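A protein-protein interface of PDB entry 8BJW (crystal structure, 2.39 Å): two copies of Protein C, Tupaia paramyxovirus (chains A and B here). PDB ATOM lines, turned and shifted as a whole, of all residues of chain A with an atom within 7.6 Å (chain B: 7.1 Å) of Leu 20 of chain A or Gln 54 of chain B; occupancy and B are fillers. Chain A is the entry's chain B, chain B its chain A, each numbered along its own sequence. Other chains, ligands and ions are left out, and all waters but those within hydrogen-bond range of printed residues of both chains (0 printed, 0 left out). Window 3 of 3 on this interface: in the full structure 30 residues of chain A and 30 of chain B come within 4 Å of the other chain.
The side-chain amide nitrogen of Gln 13 of chain A sits at hydrogen-bond distance from the backbone carbonyl oxygen of Lys 57 of chain B. The guanidinium group of Arg 50 of chain B sits at hydrogen-bond distance from the backbone carbonyl oxygen of Pro 24 of chain A, 3.5 Å away.
Of the 12 printed residues of chain A, 6 touch a printed residue of chain B. Hydrophobic or aromatic side chains of chain A within 4 Å of the printed part of chain B: Ala 16, Leu 19, Leu 20 and Leu 23. Of the 14 printed residues of chain B, 5 touch a printed residue of chain A.
Leu 20 of chain A touches four residues of chain B. Of chain A, only Leu 20 (3.7 Å) comes within 4 Å of Gln 54 of chain B. Printed residues of chain B within 4 Å of Gln 13 of chain A: Glu 56 and Lys 57. Printed residues of chain B within 4 Å of Pro 24 of chain A: Arg 50. Leu 52 of chain B touches none of the printed residues of chain A. Thr 51 of chain B touches none of the printed residues of chain A. The nearest residue of chain B that does not touch Leu 20 of chain A is Val 49 of chain B (5.8 Å).
No position is printed for both chains.
Among the printed residues, merely in contact across the chains: Gln 13 of chain A with Glu 56 of chain B (3.5 Å), Ala 16 of chain A with Leu 53 of chain B (3.6 Å), Ala 16 of chain A with Glu 56 of chain B (3.6 Å), Ala 16 of chain A with Lys 57 of chain B (3.5 Å), Leu 19 of chain A with Leu 53 of chain B (3.97 Å), Leu 20 of chain A with Arg 50 of chain B (3.96 Å), Leu 20 of chain A with Leu 53 of chain B (3.8 Å), Leu 20 of chain A with Gln 54 of chain B (3.7 Å), Leu 20 of chain A with Lys 57 of chain B (3.9 Å) and Leu 23 of chain A with Arg 50 of chain B (3.8 Å).
The side-chain amide oxygen (OE1) of Gln 54 of chain B sits close to the side-chain carboxylate (OE2) of Glu 58 of chain B, 3.0 Å away. N of Val 62 of chain B sits at hydrogen-bond distance from OE1 of Glu 56 of chain B, 2.8 Å away.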
ATOM      1  N   GLN A  13      -3.950  -9.577  24.492  1.00  0.00           N
ATOM      2  CA  GLN A  13      -3.432  -9.206  25.836  1.00  0.00           C
ATOM      3  C   GLN A  13      -2.098  -9.890  26.098  1.00  0.00           C
ATOM      4  O   GLN A  13      -1.188  -9.214  26.617  1.00  0.00           O
ATOM      5  CB  GLN A  13      -4.430  -9.564  26.931  1.00  0.00           C
ATOM      6  CG  GLN A  13      -5.690  -8.735  26.867  1.00  0.00           C
ATOM      7  CD  GLN A  13      -6.669  -9.180  27.919  1.00  0.00           C
ATOM      8  OE1 GLN A  13      -7.742  -9.672  27.609  1.00  0.00           O
ATOM      9  NE2 GLN A  13      -6.289  -9.029  29.172  1.00  0.00           N
ATOM     10  N   GLU A  14      -1.987 -11.177  25.759  1.00  0.00           N
ATOM     11  CA  GLU A  14      -0.755 -11.988  25.958  1.00  0.00           C
ATOM     12  C   GLU A  14       0.340 -11.441  25.031  1.00  0.00           C
ATOM     13  O   GLU A  14       1.484 -11.300  25.501  1.00  0.00           O
ATOM     14  CB  GLU A  14      -1.041 -13.479  25.733  1.00  0.00           C
ATOM     15  CG  GLU A  14      -2.003 -14.050  26.766  1.00  0.00           C
ATOM     16  CD  GLU A  14      -2.424 -15.505  26.606  1.00  0.00           C
ATOM     17  OE1 GLU A  14      -1.534 -16.385  26.491  1.00  0.00           O
ATOM     18  OE2 GLU A  14      -3.655 -15.756  26.598  1.00  0.00           O
ATOM     19  N   LEU A  15       0.005 -11.122  23.775  1.00  0.00           N
ATOM     20  CA  LEU A  15       0.967 -10.509  22.816  1.00  0.00           C
ATOM     21  C   LEU A  15       1.549  -9.225  23.443  1.00  0.00           C
ATOM     22  O   LEU A  15       2.782  -9.104  23.528  1.00  0.00           O
ATOM     23  CB  LEU A  15       0.262 -10.226  21.483  1.00  0.00           C
ATOM     24  CG  LEU A  15      -0.104 -11.455  20.657  1.00  0.00           C
ATOM     25  CD1 LEU A  15      -0.881 -11.047  19.406  1.00  0.00           C
ATOM     26  CD2 LEU A  15       1.120 -12.290  20.291  1.00  0.00           C
ATOM     27  N   ALA A  16       0.687  -8.343  23.943  1.00  0.00           N
ATOM     28  CA  ALA A  16       1.069  -7.074  24.611  1.00  0.00           C
ATOM     29  C   ALA A  16       1.961  -7.375  25.818  1.00  0.00           C
ATOM     30  O   ALA A  16       3.034  -6.737  25.932  1.00  0.00           O
ATOM     31  CB  ALA A  16      -0.164  -6.284  24.995  1.00  0.00           C
ATOM     32  N   GLU A  17       1.571  -8.347  26.650  1.00  0.00           N
ATOM     33  CA  GLU A  17       2.329  -8.728  27.878  1.00  0.00           C
ATOM     34  C   GLU A  17       3.732  -9.185  27.473  1.00  0.00           C
ATOM     35  O   GLU A  17       4.696  -8.827  28.180  1.00  0.00           O
ATOM     36  CB  GLU A  17       1.575  -9.820  28.640  1.00  0.00           C
ATOM     37  CG  GLU A  17       2.206 -10.266  29.959  1.00  0.00           C
ATOM     38  CD  GLU A  17       1.345 -11.305  30.682  1.00  0.00           C
ATOM     39  OE1 GLU A  17       0.091 -11.155  30.667  1.00  0.00           O
ATOM     40  OE2 GLU A  17       1.899 -12.295  31.248  1.00  0.00           O
ATOM     41  N   GLN A  18       3.843  -9.918  26.358  1.00  0.00           N
ATOM     42  CA  GLN A  18       5.133 -10.445  25.867  1.00  0.00           C
ATOM     43  C   GLN A  18       5.983  -9.278  25.332  1.00  0.00           C
ATOM     44  O   GLN A  18       7.163  -9.158  25.738  1.00  0.00           O
ATOM     45  CB  GLN A  18       4.883 -11.537  24.814  1.00  0.00           C
ATOM     46  CG  GLN A  18       6.194 -12.189  24.346  1.00  0.00           C
ATOM     47  CD  GLN A  18       7.090 -12.510  25.527  1.00  0.00           C
ATOM     48  OE1 GLN A  18       6.692 -13.258  26.416  1.00  0.00           O
ATOM     49  NE2 GLN A  18       8.283 -11.917  25.581  1.00  0.00           N
ATOM     50  N   LEU A  19       5.396  -8.422  24.483  1.00  0.00           N
ATOM     51  CA  LEU A  19       6.084  -7.218  23.951  1.00  0.00           C
ATOM     52  C   LEU A  19       6.607  -6.356  25.111  1.00  0.00           C
ATOM     53  O   LEU A  19       7.757  -5.910  25.026  1.00  0.00           O
ATOM     54  CB  LEU A  19       5.136  -6.438  23.045  1.00  0.00           C
ATOM     55  CG  LEU A  19       4.894  -7.089  21.688  1.00  0.00           C
ATOM     56  CD1 LEU A  19       3.703  -6.441  20.985  1.00  0.00           C
ATOM     57  CD2 LEU A  19       6.150  -7.033  20.832  1.00  0.00           C
ATOM     58  N   LEU A  20       5.829  -6.172  26.179  1.00  0.00           N
ATOM     59  CA  LEU A  20       6.234  -5.329  27.343  1.00  0.00           C
ATOM     60  C   LEU A  20       7.509  -5.880  27.992  1.00  0.00           C
ATOM     61  O   LEU A  20       8.344  -5.046  28.370  1.00  0.00           O
ATOM     62  CB  LEU A  20       5.086  -5.232  28.349  1.00  0.00           C
ATOM     63  CG  LEU A  20       3.984  -4.248  27.976  1.00  0.00           C
ATOM     64  CD1 LEU A  20       2.764  -4.459  28.858  1.00  0.00           C
ATOM     65  CD2 LEU A  20       4.472  -2.814  28.063  1.00  0.00           C
ATOM     66  N   LYS A  21       7.692  -7.198  28.056  1.00  0.00           N
ATOM     67  CA  LYS A  21       8.932  -7.827  28.600  1.00  0.00           C
ATOM     68  C   LYS A  21      10.101  -7.614  27.635  1.00  0.00           C
ATOM     69  O   LYS A  21      11.226  -7.411  28.131  1.00  0.00           O
ATOM     70  CB  LYS A  21       8.756  -9.321  28.861  1.00  0.00           C
ATOM     71  CG  LYS A  21       7.529  -9.697  29.687  1.00  0.00           C
ATOM     72  CD  LYS A  21       7.728  -9.799  31.187  1.00  0.00           C
ATOM     73  CE  LYS A  21       8.571 -10.982  31.630  1.00  0.00           C
ATOM     74  NZ  LYS A  21       8.368 -11.276  33.068  1.00  0.00           N
ATOM     75  N   GLU A  22       9.854  -7.600  26.325  1.00  0.00           N
ATOM     76  CA  GLU A  22      10.898  -7.480  25.275  1.00  0.00           C
ATOM     77  C   GLU A  22      11.333  -6.014  25.050  1.00  0.00           C
ATOM     78  O   GLU A  22      12.316  -5.793  24.305  1.00  0.00           O
ATOM     79  CB  GLU A  22      10.380  -8.108  23.980  1.00  0.00           C
ATOM     80  CG  GLU A  22      10.439  -9.631  23.970  1.00  0.00           C
ATOM     81  CD  GLU A  22       9.627 -10.300  22.870  1.00  0.00           C
ATOM     82  OE1 GLU A  22       8.946  -9.562  22.086  1.00  0.00           O
ATOM     83  OE2 GLU A  22       9.636 -11.550  22.821  1.00  0.00           O
ATOM     84  N   LEU A  23      10.600  -5.015  25.567  1.00  0.00           N
ATOM     85  CA  LEU A  23      10.892  -3.563  25.334  1.00  0.00           C
ATOM     86  C   LEU A  23      12.235  -3.221  25.949  1.00  0.00           C
ATOM     87  O   LEU A  23      12.549  -3.669  27.040  1.00  0.00           O
ATOM     88  CB  LEU A  23       9.811  -2.661  25.943  1.00  0.00           C
ATOM     89  CG  LEU A  23       8.500  -2.580  25.163  1.00  0.00           C
ATOM     90  CD1 LEU A  23       7.577  -1.569  25.796  1.00  0.00           C
ATOM     91  CD2 LEU A  23       8.715  -2.209  23.705  1.00  0.00           C
ATOM     92  N   PRO A  24      13.044  -2.373  25.277  1.00  0.00           N
ATOM     93  CA  PRO A  24      14.328  -1.958  25.822  1.00  0.00           C
ATOM     94  C   PRO A  24      14.104  -1.373  27.224  1.00  0.00           C
ATOM     95  O   PRO A  24      13.006  -0.861  27.497  1.00  0.00           O
ATOM     96  CB  PRO A  24      14.887  -0.928  24.818  1.00  0.00           C
ATOM     97  CG  PRO A  24      13.700  -0.551  23.921  1.00  0.00           C
ATOM     98  CD  PRO A  24      12.740  -1.720  23.987  1.00  0.00           C
ATOM     99  N   LEU B  48       5.227   6.448  25.207  1.00  0.00           N
ATOM    100  CA  LEU B  48       3.861   6.358  24.648  1.00  0.00           C
ATOM    101  C   LEU B  48       3.623   4.922  24.162  1.00  0.00           C
ATOM    102  O   LEU B  48       2.545   4.394  24.368  1.00  0.00           O
ATOM    103  CB  LEU B  48       3.705   7.366  23.501  1.00  0.00           C
ATOM    104  CG  LEU B  48       2.993   8.647  23.899  1.00  0.00           C
ATOM    105  CD1 LEU B  48       2.880   9.608  22.726  1.00  0.00           C
ATOM    106  CD2 LEU B  48       1.632   8.321  24.479  1.00  0.00           C
ATOM    107  N   VAL B  49       4.606   4.333  23.511  1.00  0.00           N
ATOM    108  CA  VAL B  49       4.528   2.941  23.015  1.00  0.00           C
ATOM    109  C   VAL B  49       4.235   2.018  24.204  1.00  0.00           C
ATOM    110  O   VAL B  49       3.275   1.220  24.103  1.00  0.00           O
ATOM    111  CB  VAL B  49       5.810   2.550  22.280  1.00  0.00           C
ATOM    112  CG1 VAL B  49       5.916   1.052  22.106  1.00  0.00           C
ATOM    113  CG2 VAL B  49       5.905   3.285  20.955  1.00  0.00           C
ATOM    114  N   ARG B  50       4.982   2.185  25.298  1.00  0.00           N
ATOM    115  CA  ARG B  50       4.810   1.404  26.543  1.00  0.00           C
ATOM    116  C   ARG B  50       3.388   1.650  27.070  1.00  0.00           C
ATOM    117  O   ARG B  50       2.710   0.674  27.412  1.00  0.00           O
ATOM    118  CB  ARG B  50       5.913   1.738  27.561  1.00  0.00           C
ATOM    119  CG  ARG B  50       5.722   0.993  28.882  1.00  0.00           C
ATOM    120  CD  ARG B  50       6.770   1.158  29.970  1.00  0.00           C
ATOM    121  NE  ARG B  50       8.118   0.847  29.484  1.00  0.00           N
ATOM    122  CZ  ARG B  50       8.727  -0.338  29.550  1.00  0.00           C
ATOM    123  NH1 ARG B  50       8.114  -1.387  30.075  1.00  0.00           N
ATOM    124  NH2 ARG B  50       9.955  -0.470  29.078  1.00  0.00           N
ATOM    125  N   THR B  51       2.918   2.898  27.146  1.00  0.00           N
ATOM    126  CA  THR B  51       1.561   3.233  27.657  1.00  0.00           C
ATOM    127  C   THR B  51       0.524   2.518  26.799  1.00  0.00           C
ATOM    128  O   THR B  51      -0.390   1.933  27.371  1.00  0.00           O
ATOM    129  CB  THR B  51       1.326   4.745  27.652  1.00  0.00           C
ATOM    130  OG1 THR B  51       2.318   5.255  28.542  1.00  0.00           O
ATOM    131  CG2 THR B  51      -0.062   5.162  28.103  1.00  0.00           C
ATOM    132  N   LEU B  52       0.653   2.553  25.470  1.00  0.00           N
ATOM    133  CA  LEU B  52      -0.333   1.925  24.568  1.00  0.00           C
ATOM    134  C   LEU B  52      -0.306   0.402  24.765  1.00  0.00           C
ATOM    135  O   LEU B  52      -1.376  -0.177  24.842  1.00  0.00           O
ATOM    136  CB  LEU B  52      -0.052   2.341  23.124  1.00  0.00           C
ATOM    137  CG  LEU B  52      -0.427   3.778  22.767  1.00  0.00           C
ATOM    138  CD1 LEU B  52      -0.119   4.065  21.321  1.00  0.00           C
ATOM    139  CD2 LEU B  52      -1.908   4.053  23.024  1.00  0.00           C
ATOM    140  N   LEU B  53       0.869  -0.215  24.888  1.00  0.00           N
ATOM    141  CA  LEU B  53       0.957  -1.676  25.117  1.00  0.00           C
ATOM    142  C   LEU B  53       0.374  -2.016  26.505  1.00  0.00           C
ATOM    143  O   LEU B  53      -0.283  -3.077  26.616  1.00  0.00           O
ATOM    144  CB  LEU B  53       2.409  -2.131  24.968  1.00  0.00           C
ATOM    145  CG  LEU B  53       2.913  -2.175  23.530  1.00  0.00           C
ATOM    146  CD1 LEU B  53       4.416  -2.441  23.468  1.00  0.00           C
ATOM    147  CD2 LEU B  53       2.162  -3.216  22.720  1.00  0.00           C
ATOM    148  N   GLN B  54       0.586  -1.183  27.528  1.00  0.00           N
ATOM    149  CA  GLN B  54      -0.031  -1.395  28.867  1.00  0.00           C
ATOM    150  C   GLN B  54      -1.550  -1.452  28.699  1.00  0.00           C
ATOM    151  O   GLN B  54      -2.173  -2.359  29.266  1.00  0.00           O
ATOM    152  CB  GLN B  54       0.355  -0.321  29.885  1.00  0.00           C
ATOM    153  CG  GLN B  54       1.253  -0.804  31.038  1.00  0.00           C
ATOM    154  CD  GLN B  54       0.819  -2.104  31.699  1.00  0.00           C
ATOM    155  OE1 GLN B  54      -0.361  -2.366  31.969  1.00  0.00           O
ATOM    156  NE2 GLN B  54       1.811  -2.910  32.054  1.00  0.00           N
ATOM    157  N   MET B  55      -2.128  -0.571  27.886  1.00  0.00           N
ATOM    158  CA  MET B  55      -3.583  -0.563  27.606  1.00  0.00           C
ATOM    159  C   MET B  55      -3.991  -1.874  26.943  1.00  0.00           C
ATOM    160  O   MET B  55      -5.029  -2.427  27.347  1.00  0.00           O
ATOM    161  CB  MET B  55      -3.975   0.613  26.697  1.00  0.00           C
ATOM    162  CG  MET B  55      -3.811   1.934  27.397  1.00  0.00           C
ATOM    163  SD  MET B  55      -4.133   3.405  26.446  1.00  0.00           S
ATOM    164  CE  MET B  55      -5.781   3.110  25.806  1.00  0.00           C
ATOM    165  N   GLU B  56      -3.271  -2.316  25.918  1.00  0.00           N
ATOM    166  CA  GLU B  56      -3.533  -3.575  25.179  1.00  0.00           C
ATOM    167  C   GLU B  56      -3.511  -4.731  26.183  1.00  0.00           C
ATOM    168  O   GLU B  56      -4.475  -5.526  26.194  1.00  0.00           O
ATOM    169  CB  GLU B  56      -2.523  -3.755  24.058  1.00  0.00           C
ATOM    170  CG  GLU B  56      -2.873  -4.881  23.083  1.00  0.00           C
ATOM    171  CD  GLU B  56      -3.925  -4.485  22.063  1.00  0.00           C
ATOM    172  OE1 GLU B  56      -3.818  -3.354  21.509  1.00  0.00           O
ATOM    173  OE2 GLU B  56      -4.857  -5.314  21.824  1.00  0.00           O
ATOM    174  N   LYS B  57      -2.500  -4.773  27.047  1.00  0.00           N
ATOM    175  CA  LYS B  57      -2.394  -5.846  28.067  1.00  0.00           C
ATOM    176  C   LYS B  57      -3.643  -5.851  28.965  1.00  0.00           C
ATOM    177  O   LYS B  57      -4.124  -6.937  29.283  1.00  0.00           O
ATOM    178  CB  LYS B  57      -1.115  -5.689  28.888  1.00  0.00           C
ATOM    179  CG  LYS B  57      -0.992  -6.675  30.045  1.00  0.00           C
ATOM    180  CD  LYS B  57       0.047  -6.269  31.039  1.00  0.00           C
ATOM    181  CE  LYS B  57       0.035  -7.163  32.256  1.00  0.00           C
ATOM    182  NZ  LYS B  57       1.408  -7.383  32.774  1.00  0.00           N
ATOM    183  N   GLU B  58      -4.124  -4.671  29.366  1.00  0.00           N
ATOM    184  CA  GLU B  58      -5.255  -4.513  30.313  1.00  0.00           C
ATOM    185  C   GLU B  58      -6.590  -4.825  29.623  1.00  0.00           C
ATOM    186  O   GLU B  58      -7.576  -4.939  30.345  1.00  0.00           O
ATOM    187  CB  GLU B  58      -5.264  -3.107  30.918  1.00  0.00           C
ATOM    188  CG  GLU B  58      -4.284  -2.931  32.050  1.00  0.00           C
ATOM    189  CD  GLU B  58      -3.861  -1.493  32.325  1.00  0.00           C
ATOM    190  OE1 GLU B  58      -4.422  -0.567  31.669  1.00  0.00           O
ATOM    191  OE2 GLU B  58      -2.907  -1.296  33.123  1.00  0.00           O
ATOM    192  N   GLY B  59      -6.627  -4.972  28.299  1.00  0.00           N
ATOM    193  CA  GLY B  59      -7.847  -5.352  27.558  1.00  0.00           C
ATOM    194  C   GLY B  59      -8.445  -4.210  26.748  1.00  0.00           C
ATOM    195  O   GLY B  59      -9.523  -4.403  26.148  1.00  0.00           O
ATOM    196  N   THR B  60      -7.781  -3.057  26.694  1.00  0.00           N
ATOM    197  CA  THR B  60      -8.170  -1.931  25.804  1.00  0.00           C
ATOM    198  C   THR B  60      -7.429  -2.120  24.481  1.00  0.00           C
ATOM    199  O   THR B  60      -6.227  -1.817  24.447  1.00  0.00           O
ATOM    200  CB  THR B  60      -7.858  -0.566  26.435  1.00  0.00           C
ATOM    201  OG1 THR B  60      -8.400  -0.456  27.742  1.00  0.00           O
ATOM    202  CG2 THR B  60      -8.374   0.575  25.597  1.00  0.00           C
ATOM    203  N   VAL B  62      -5.843  -1.514  20.997  1.00  0.00           N
ATOM    204  CA  VAL B  62      -5.306  -0.234  20.471  1.00  0.00           C
ATOM    205  C   VAL B  62      -5.665  -0.137  18.991  1.00  0.00           C
ATOM    206  O   VAL B  62      -5.101  -0.893  18.201  1.00  0.00           O
ATOM    207  CB  VAL B  62      -3.799  -0.091  20.763  1.00  0.00           C
ATOM    208  CG1 VAL B  62      -3.194   1.138  20.097  1.00  0.00           C
ATOM    209  CG2 VAL B  62      -3.544  -0.068  22.262  1.00  0.00           C
